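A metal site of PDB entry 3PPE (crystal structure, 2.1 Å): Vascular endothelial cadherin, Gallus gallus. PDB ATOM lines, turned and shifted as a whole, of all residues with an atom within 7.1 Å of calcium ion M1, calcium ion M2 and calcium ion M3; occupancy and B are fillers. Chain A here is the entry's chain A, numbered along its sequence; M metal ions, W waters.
Calcium ion M2 is bound by the side-chain carboxylate (OD1) of Asp 99 (2.2 Å), the side-chain carboxylate (OE2) of Glu 11 (2.3 Å), the side-chain carboxylate (OD2) of Asp 96 (2.3 Å), the backbone carbonyl oxygen (O) of Ile 97 (2.4 Å), the side-chain carboxylate (OD1) of Asp 132 (2.4 Å), the side-chain carboxylate (OE2) of Glu 64 (2.5 Å) and the side-chain carboxylate (OE1) of Glu 64 (2.7 Å). Calcium ion M2 has seven donor atoms within binding distance.
The side-chain carboxylate (OE1) of Glu 11 sits close to the backbone NH (N) of Arg 63 (2.9 Å). The backbone NH of Asp 133 sits at hydrogen-bond distance from the side-chain carboxylate of Asp 96, at 3.0 Å. The backbone NH (N) of Leu 186 sits close to the side-chain carboxylate (OD2) of Asp 184 (3.0 Å). The backbone NH (N) of Leu 188 lies within hydrogen-bond range of the side-chain carboxylate (OD2) of Asp 184. The backbone NH (N) of Glu 12 sits at hydrogen-bond distance from the backbone carbonyl oxygen (O) of Leu 61. The side-chain carboxylate of Glu 64 lies close to the guanidinium group of Arg 63. ND1 of His 139 lies within hydrogen-bond range of OD1 of Asp 96 (2.8 Å). OE2 of Glu 12 lies within salt-bridge range of NH2 of Arg 60.
Within 4 Å of calcium ion M1: Asn 98, Asn 100, Asp 130, Asp 132, His 139 and Asp 184. The nearest printed residue that does not touch calcium ion M1 is Leu 188 (4.4 Å).
Seven residues have an atom within 4 Å of calcium ion M2: Glu 11, Glu 64, Asp 96, Ile 97, Asp 99, Asn 100 and Asp 132. The nearest printed residue that does not touch calcium ion M2 is Arg 63 (4.3 Å).
Calcium ion M3 is bound by OD1 of Asp 62, OE1 of Glu 64, OD2 of Asp 99, OE1 of Glu 11, water W1 and OE1 of Glu 12.
Calcium ion M1 is bound by the backbone carbonyl oxygen (O) of His 139 (2.3 Å), the backbone carbonyl oxygen (O) of Asn 100 (2.3 Å), the side-chain carboxylate (OD2) of Asp 132 (2.4 Å), the side-chain amide oxygen (OD1) of Asn 98 (2.4 Å), the side-chain carboxylate (OD2) of Asp 130 (2.4 Å), the side-chain carboxylate (OD1) of Asp 130 (2.6 Å) and the side-chain carboxylate (OD1) of Asp 184 (2.6 Å). Calcium ion M1 has seven donor atoms within binding distance.
Five residues have an atom within 4 Å of calcium ion M3: Glu 11, Glu 12, Asp 62, Glu 64 and Asp 99.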
ATOM      1  N   GLU A  11      22.741  34.250 -12.945  1.00  0.00           N
ATOM      2  CA  GLU A  11      22.567  33.455 -14.155  1.00  0.00           C
ATOM      3  C   GLU A  11      21.157  32.935 -14.250  1.00  0.00           C
ATOM      4  O   GLU A  11      20.447  32.852 -13.239  1.00  0.00           O
ATOM      5  CB  GLU A  11      23.555  32.273 -14.196  1.00  0.00           C
ATOM      6  CG  GLU A  11      23.320  31.294 -13.042  1.00  0.00           C
ATOM      7  CD  GLU A  11      23.961  29.924 -13.260  1.00  0.00           C
ATOM      8  OE1 GLU A  11      24.134  29.507 -14.430  1.00  0.00           O
ATOM      9  OE2 GLU A  11      24.287  29.279 -12.246  1.00  0.00           O
ATOM     10  N   GLU A  12      20.759  32.584 -15.477  1.00  0.00           N
ATOM     11  CA  GLU A  12      19.501  31.823 -15.749  1.00  0.00           C
ATOM     12  C   GLU A  12      18.212  32.583 -15.347  1.00  0.00           C
ATOM     13  O   GLU A  12      17.219  31.987 -14.945  1.00  0.00           O
ATOM     14  CB  GLU A  12      19.537  30.438 -15.073  1.00  0.00           C
ATOM     15  CG  GLU A  12      20.829  29.635 -15.288  1.00  0.00           C
ATOM     16  CD  GLU A  12      21.068  29.137 -16.705  1.00  0.00           C
ATOM     17  OE1 GLU A  12      22.036  28.373 -16.884  1.00  0.00           O
ATOM     18  OE2 GLU A  12      20.347  29.476 -17.671  1.00  0.00           O
ATOM     19  N   ARG A  60      19.874  35.736 -21.538  1.00  0.00           N
ATOM     20  CA  ARG A  60      19.989  34.947 -20.330  1.00  0.00           C
ATOM     21  C   ARG A  60      21.403  34.373 -20.282  1.00  0.00           C
ATOM     22  O   ARG A  60      21.959  33.974 -21.327  1.00  0.00           O
ATOM     23  CB  ARG A  60      18.986  33.804 -20.327  1.00  0.00           C
ATOM     24  CG  ARG A  60      17.567  34.257 -20.121  1.00  0.00           C
ATOM     25  CD  ARG A  60      16.652  33.047 -20.076  1.00  0.00           C
ATOM     26  NE  ARG A  60      17.124  32.112 -19.052  1.00  0.00           N
ATOM     27  CZ  ARG A  60      17.736  30.950 -19.281  1.00  0.00           C
ATOM     28  NH1 ARG A  60      17.962  30.504 -20.521  1.00  0.00           N
ATOM     29  NH2 ARG A  60      18.107  30.216 -18.252  1.00  0.00           N
ATOM     30  N   LEU A  61      21.975  34.333 -19.093  1.00  0.00           N
ATOM     31  CA  LEU A  61      23.350  33.946 -18.893  1.00  0.00           C
ATOM     32  C   LEU A  61      23.495  32.569 -18.166  1.00  0.00           C
ATOM     33  O   LEU A  61      22.712  32.228 -17.303  1.00  0.00           O
ATOM     34  CB  LEU A  61      24.073  35.039 -18.078  1.00  0.00           C
ATOM     35  CG  LEU A  61      24.041  36.455 -18.674  1.00  0.00           C
ATOM     36  CD1 LEU A  61      24.537  37.480 -17.653  1.00  0.00           C
ATOM     37  CD2 LEU A  61      24.824  36.498 -19.995  1.00  0.00           C
ATOM     38  N   ASP A  62      24.528  31.836 -18.519  1.00  0.00           N
ATOM     39  CA  ASP A  62      24.812  30.573 -17.854  1.00  0.00           C
ATOM     40  C   ASP A  62      26.194  30.689 -17.283  1.00  0.00           C
ATOM     41  O   ASP A  62      27.152  30.709 -18.026  1.00  0.00           O
ATOM     42  CB  ASP A  62      24.760  29.454 -18.903  1.00  0.00           C
ATOM     43  CG  ASP A  62      25.022  28.077 -18.316  1.00  0.00           C
ATOM     44  OD1 ASP A  62      25.174  27.909 -17.077  1.00  0.00           O
ATOM     45  OD2 ASP A  62      25.085  27.153 -19.132  1.00  0.00           O
ATOM     46  N   ARG A  63      26.292  30.781 -15.963  1.00  0.00           N
ATOM     47  CA  ARG A  63      27.619  30.833 -15.296  1.00  0.00           C
ATOM     48  C   ARG A  63      28.522  29.634 -15.679  1.00  0.00           C
ATOM     49  O   ARG A  63      29.747  29.761 -15.743  1.00  0.00           O
ATOM     50  CB  ARG A  63      27.462  30.935 -13.770  1.00  0.00           C
ATOM     51  CG  ARG A  63      28.730  31.348 -13.041  1.00  0.00           C
ATOM     52  CD  ARG A  63      28.715  30.774 -11.609  1.00  0.00           C
ATOM     53  NE  ARG A  63      28.803  29.287 -11.651  1.00  0.00           N
ATOM     54  CZ  ARG A  63      29.952  28.618 -11.761  1.00  0.00           C
ATOM     55  NH1 ARG A  63      31.086  29.276 -11.833  1.00  0.00           N
ATOM     56  NH2 ARG A  63      29.963  27.290 -11.851  1.00  0.00           N
ATOM     57  N   GLU A  64      27.909  28.495 -15.948  1.00  0.00           N
ATOM     58  CA  GLU A  64      28.689  27.309 -16.295  1.00  0.00           C
ATOM     59  C   GLU A  64      29.286  27.358 -17.704  1.00  0.00           C
ATOM     60  O   GLU A  64      30.187  26.581 -18.029  1.00  0.00           O
ATOM     61  CB  GLU A  64      27.859  26.028 -16.095  1.00  0.00           C
ATOM     62  CG  GLU A  64      27.735  25.608 -14.625  1.00  0.00           C
ATOM     63  CD  GLU A  64      26.812  26.473 -13.801  1.00  0.00           C
ATOM     64  OE1 GLU A  64      25.632  26.697 -14.174  1.00  0.00           O
ATOM     65  OE2 GLU A  64      27.257  26.932 -12.726  1.00  0.00           O
ATOM     66  N   LYS A  65      28.802  28.288 -18.536  1.00  0.00           N
ATOM     67  CA  LYS A  65      29.405  28.578 -19.850  1.00  0.00           C
ATOM     68  C   LYS A  65      30.490  29.659 -19.708  1.00  0.00           C
ATOM     69  O   LYS A  65      31.618  29.495 -20.178  1.00  0.00           O
ATOM     70  CB  LYS A  65      28.322  29.162 -20.722  1.00  0.00           C
ATOM     71  CG  LYS A  65      28.115  28.514 -22.052  1.00  0.00           C
ATOM     72  CD  LYS A  65      27.339  27.200 -21.890  1.00  0.00           C
ATOM     73  CE  LYS A  65      26.475  26.909 -23.121  1.00  0.00           C
ATOM     74  NZ  LYS A  65      26.488  25.449 -23.446  1.00  0.00           N
ATOM     75  N   SER A  95      26.518  35.527 -11.080  1.00  0.00           N
ATOM     76  CA  SER A  95      26.280  34.916  -9.772  1.00  0.00           C
ATOM     77  C   SER A  95      25.623  33.556  -9.971  1.00  0.00           C
ATOM     78  O   SER A  95      24.672  33.431 -10.711  1.00  0.00           O
ATOM     79  CB  SER A  95      25.345  35.791  -8.920  1.00  0.00           C
ATOM     80  OG  SER A  95      25.853  37.118  -8.881  1.00  0.00           O
ATOM     81  N   ASP A  96      26.138  32.556  -9.281  1.00  0.00           N
ATOM     82  CA  ASP A  96      25.728  31.162  -9.428  1.00  0.00           C
ATOM     83  C   ASP A  96      24.355  30.854  -8.838  1.00  0.00           C
ATOM     84  O   ASP A  96      24.076  31.220  -7.704  1.00  0.00           O
ATOM     85  CB  ASP A  96      26.768  30.278  -8.705  1.00  0.00           C
ATOM     86  CG  ASP A  96      26.629  28.813  -9.049  1.00  0.00           C
ATOM     87  OD1 ASP A  96      26.659  27.974  -8.110  1.00  0.00           O
ATOM     88  OD2 ASP A  96      26.496  28.459 -10.244  1.00  0.00           O
ATOM     89  N   ILE A  97      23.526  30.133  -9.569  1.00  0.00           N
ATOM     90  CA  ILE A  97      22.410  29.455  -8.940  1.00  0.00           C
ATOM     91  C   ILE A  97      22.726  27.953  -8.895  1.00  0.00           C
ATOM     92  O   ILE A  97      23.549  27.443  -9.675  1.00  0.00           O
ATOM     93  CB  ILE A  97      21.020  29.755  -9.637  1.00  0.00           C
ATOM     94  CG1 ILE A  97      20.883  29.105 -11.024  1.00  0.00           C
ATOM     95  CG2 ILE A  97      20.717  31.320  -9.653  1.00  0.00           C
ATOM     96  CD1 ILE A  97      19.400  28.933 -11.488  1.00  0.00           C
ATOM     97  N   ASN A  98      22.061  27.249  -7.991  1.00  0.00           N
ATOM     98  CA  ASN A  98      22.200  25.806  -7.924  1.00  0.00           C
ATOM     99  C   ASN A  98      21.372  25.129  -9.027  1.00  0.00           C
ATOM    100  O   ASN A  98      20.214  24.806  -8.842  1.00  0.00           O
ATOM    101  CB  ASN A  98      21.840  25.266  -6.533  1.00  0.00           C
ATOM    102  CG  ASN A  98      22.358  23.850  -6.352  1.00  0.00           C
ATOM    103  OD1 ASN A  98      23.491  23.548  -6.800  1.00  0.00           O
ATOM    104  ND2 ASN A  98      21.570  22.971  -5.796  1.00  0.00           N
ATOM    105  N   ASP A  99      21.959  24.944 -10.195  1.00  0.00           N
ATOM    106  CA  ASP A  99      21.218  24.371 -11.299  1.00  0.00           C
ATOM    107  C   ASP A  99      21.864  23.117 -11.913  1.00  0.00           C
ATOM    108  O   ASP A  99      21.458  22.665 -12.960  1.00  0.00           O
ATOM    109  CB  ASP A  99      20.884  25.436 -12.367  1.00  0.00           C
ATOM    110  CG  ASP A  99      22.108  26.128 -12.966  1.00  0.00           C
ATOM    111  OD1 ASP A  99      23.206  26.190 -12.355  1.00  0.00           O
ATOM    112  OD2 ASP A  99      21.953  26.676 -14.112  1.00  0.00           O
ATOM    113  N   ASN A 100      22.884  22.575 -11.230  1.00  0.00           N
ATOM    114  CA  ASN A 100      23.520  21.345 -11.634  1.00  0.00           C
ATOM    115  C   ASN A 100      23.547  20.325 -10.507  1.00  0.00           C
ATOM    116  O   ASN A 100      23.759  20.655  -9.325  1.00  0.00           O
ATOM    117  CB  ASN A 100      24.957  21.583 -12.176  1.00  0.00           C
ATOM    118  CG  ASN A 100      24.979  22.451 -13.434  1.00  0.00           C
ATOM    119  OD1 ASN A 100      24.976  23.676 -13.345  1.00  0.00           O
ATOM    120  ND2 ASN A 100      24.940  21.825 -14.600  1.00  0.00           N
ATOM    121  N   ALA A 101      23.314  19.074 -10.866  1.00  0.00           N
ATOM    122  CA  ALA A 101      23.436  17.985  -9.899  1.00  0.00           C
ATOM    123  C   ALA A 101      24.845  17.354 -10.053  1.00  0.00           C
ATOM    124  O   ALA A 101      25.514  17.540 -11.080  1.00  0.00           O
ATOM    125  CB  ALA A 101      22.324  16.943 -10.120  1.00  0.00           C
ATOM    126  N   PRO A 102      25.342  16.682  -9.003  1.00  0.00           N
ATOM    127  CA  PRO A 102      26.632  15.966  -9.194  1.00  0.00           C
ATOM    128  C   PRO A 102      26.456  14.819 -10.173  1.00  0.00           C
ATOM    129  O   PRO A 102      25.390  14.129 -10.177  1.00  0.00           O
ATOM    130  CB  PRO A 102      26.962  15.443  -7.780  1.00  0.00           C
ATOM    131  CG  PRO A 102      26.058  16.329  -6.851  1.00  0.00           C
ATOM    132  CD  PRO A 102      24.806  16.517  -7.645  1.00  0.00           C
ATOM    133  N   ASP A 130      30.130  18.294  -9.459  1.00  0.00           N
ATOM    134  CA  ASP A 130      28.964  19.161  -9.572  1.00  0.00           C
ATOM    135  C   ASP A 130      29.482  20.440 -10.212  1.00  0.00           C
ATOM    136  O   ASP A 130      30.398  21.056  -9.680  1.00  0.00           O
ATOM    137  CB  ASP A 130      28.433  19.451  -8.187  1.00  0.00           C
ATOM    138  CG  ASP A 130      27.130  20.212  -8.206  1.00  0.00           C
ATOM    139  OD1 ASP A 130      27.015  21.306  -8.814  1.00  0.00           O
ATOM    140  OD2 ASP A 130      26.223  19.753  -7.522  1.00  0.00           O
ATOM    141  N   ALA A 131      28.862  20.824 -11.336  1.00  0.00           N
ATOM    142  CA  ALA A 131      29.341  21.931 -12.164  1.00  0.00           C
ATOM    143  C   ALA A 131      29.059  23.339 -11.592  1.00  0.00           C
ATOM    144  O   ALA A 131      29.537  24.348 -12.128  1.00  0.00           O
ATOM    145  CB  ALA A 131      28.731  21.798 -13.542  1.00  0.00           C
ATOM    146  N   ASP A 132      28.286  23.423 -10.515  1.00  0.00           N
ATOM    147  CA  ASP A 132      28.019  24.702  -9.858  1.00  0.00           C
ATOM    148  C   ASP A 132      29.280  25.266  -9.193  1.00  0.00           C
ATOM    149  O   ASP A 132      30.337  24.614  -9.169  1.00  0.00           O
ATOM    150  CB  ASP A 132      26.817  24.617  -8.893  1.00  0.00           C
ATOM    151  CG  ASP A 132      25.548  24.298  -9.631  1.00  0.00           C
ATOM    152  OD1 ASP A 132      25.305  24.948 -10.649  1.00  0.00           O
ATOM    153  OD2 ASP A 132      24.777  23.374  -9.231  1.00  0.00           O
ATOM    154  N   ASP A 133      29.155  26.467  -8.656  1.00  0.00           N
ATOM    155  CA  ASP A 133      30.305  27.181  -8.095  1.00  0.00           C
ATOM    156  C   ASP A 133      30.636  26.679  -6.693  1.00  0.00           C
ATOM    157  O   ASP A 133      29.801  26.747  -5.789  1.00  0.00           O
ATOM    158  CB  ASP A 133      30.040  28.682  -8.069  1.00  0.00           C
ATOM    159  CG  ASP A 133      31.281  29.485  -7.711  1.00  0.00           C
ATOM    160  OD1 ASP A 133      31.301  30.700  -7.975  1.00  0.00           O
ATOM    161  OD2 ASP A 133      32.232  28.895  -7.161  1.00  0.00           O
ATOM    162  N   GLY A 138      27.253  25.630  -0.718  1.00  0.00           N
ATOM    163  CA  GLY A 138      26.771  24.269  -0.769  1.00  0.00           C
ATOM    164  C   GLY A 138      26.482  23.815  -2.192  1.00  0.00           C
ATOM    165  O   GLY A 138      26.150  22.647  -2.423  1.00  0.00           O
ATOM    166  N   HIS A 139      26.595  24.733  -3.140  1.00  0.00           N
ATOM    167  CA  HIS A 139      26.072  24.519  -4.484  1.00  0.00           C
ATOM    168  C   HIS A 139      26.765  23.353  -5.167  1.00  0.00           C
ATOM    169  O   HIS A 139      26.150  22.636  -5.959  1.00  0.00           O
ATOM    170  CB  HIS A 139      26.234  25.792  -5.327  1.00  0.00           C
ATOM    171  CG  HIS A 139      25.203  26.840  -5.039  1.00  0.00           C
ATOM    172  ND1 HIS A 139      24.962  27.900  -5.884  1.00  0.00           N
ATOM    173  CD2 HIS A 139      24.341  26.992  -3.994  1.00  0.00           C
ATOM    174  CE1 HIS A 139      24.012  28.658  -5.383  1.00  0.00           C
ATOM    175  NE2 HIS A 139      23.618  28.130  -4.235  1.00  0.00           N
ATOM    176  N   ALA A 140      28.045  23.156  -4.858  1.00  0.00           N
ATOM    177  CA  ALA A 140      28.819  22.085  -5.451  1.00  0.00           C
ATOM    178  C   ALA A 140      29.276  21.134  -4.337  1.00  0.00           C
ATOM    179  O   ALA A 140      30.291  20.435  -4.471  1.00  0.00           O
ATOM    180  CB  ALA A 140      29.987  22.670  -6.165  1.00  0.00           C
ATOM    181  N   THR A 141      28.551  21.108  -3.241  1.00  0.00           N
ATOM    182  CA  THR A 141      28.855  20.209  -2.161  1.00  0.00           C
ATOM    183  C   THR A 141      28.207  18.850  -2.501  1.00  0.00           C
ATOM    184  O   THR A 141      26.987  18.767  -2.593  1.00  0.00           O
ATOM    185  CB  THR A 141      28.248  20.715  -0.838  1.00  0.00           C
ATOM    186  OG1 THR A 141      28.846  21.963  -0.468  1.00  0.00           O
ATOM    187  CG2 THR A 141      28.531  19.729   0.296  1.00  0.00           C
ATOM    188  N   ASP A 184      23.839  16.939  -4.301  1.00  0.00           N
ATOM    189  CA  ASP A 184      24.421  18.120  -3.674  1.00  0.00           C
ATOM    190  C   ASP A 184      23.613  18.548  -2.455  1.00  0.00           C
ATOM    191  O   ASP A 184      22.464  18.143  -2.283  1.00  0.00           O
ATOM    192  CB  ASP A 184      24.504  19.273  -4.676  1.00  0.00           C
ATOM    193  CG  ASP A 184      23.165  19.910  -4.949  1.00  0.00           C
ATOM    194  OD1 ASP A 184      23.022  20.611  -5.972  1.00  0.00           O
ATOM    195  OD2 ASP A 184      22.236  19.706  -4.135  1.00  0.00           O
ATOM    196  N   ALA A 185      24.227  19.362  -1.599  1.00  0.00           N
ATOM    197  CA  ALA A 185      23.751  19.539  -0.235  1.00  0.00           C
ATOM    198  C   ALA A 185      22.387  20.220  -0.210  1.00  0.00           C
ATOM    199  O   ALA A 185      21.708  20.232   0.811  1.00  0.00           O
ATOM    200  CB  ALA A 185      24.756  20.342   0.576  1.00  0.00           C
ATOM    201  N   LEU A 186      21.991  20.782  -1.353  1.00  0.00           N
ATOM    202  CA  LEU A 186      20.695  21.430  -1.475  1.00  0.00           C
ATOM    203  C   LEU A 186      19.650  20.491  -2.049  1.00  0.00           C
ATOM    204  O   LEU A 186      18.474  20.833  -2.154  1.00  0.00           O
ATOM    205  CB  LEU A 186      20.807  22.691  -2.337  1.00  0.00           C
ATOM    206  CG  LEU A 186      21.487  23.902  -1.693  1.00  0.00           C
ATOM    207  CD1 LEU A 186      22.993  23.727  -1.699  1.00  0.00           C
ATOM    208  CD2 LEU A 186      21.087  25.188  -2.413  1.00  0.00           C
ATOM    209  N   LEU A 188      19.880  18.496  -4.968  1.00  0.00           N
ATOM    210  CA  LEU A 188      19.771  18.358  -6.420  1.00  0.00           C
ATOM    211  C   LEU A 188      20.301  17.010  -6.886  1.00  0.00           C
ATOM    212  O   LEU A 188      21.487  16.724  -6.773  1.00  0.00           O
ATOM    213  CB  LEU A 188      20.529  19.491  -7.114  1.00  0.00           C
ATOM    214  CG  LEU A 188      19.787  20.204  -8.256  1.00  0.00           C
ATOM    215  CD1 LEU A 188      18.391  20.625  -7.807  1.00  0.00           C
ATOM    216  CD2 LEU A 188      20.582  21.401  -8.753  1.00  0.00           C
HETATM  217 CA    CA M   1      24.794  21.711  -7.556  1.00  0.00          CA
HETATM  218 CA    CA M   2      25.039  27.189 -11.548  1.00  0.00          CA
HETATM  219 CA    CA M   3      23.776  27.379 -15.370  1.00  0.00          CA
HETATM  220  O   HOH W   1      23.692  25.003 -16.031  1.00  0.00           O
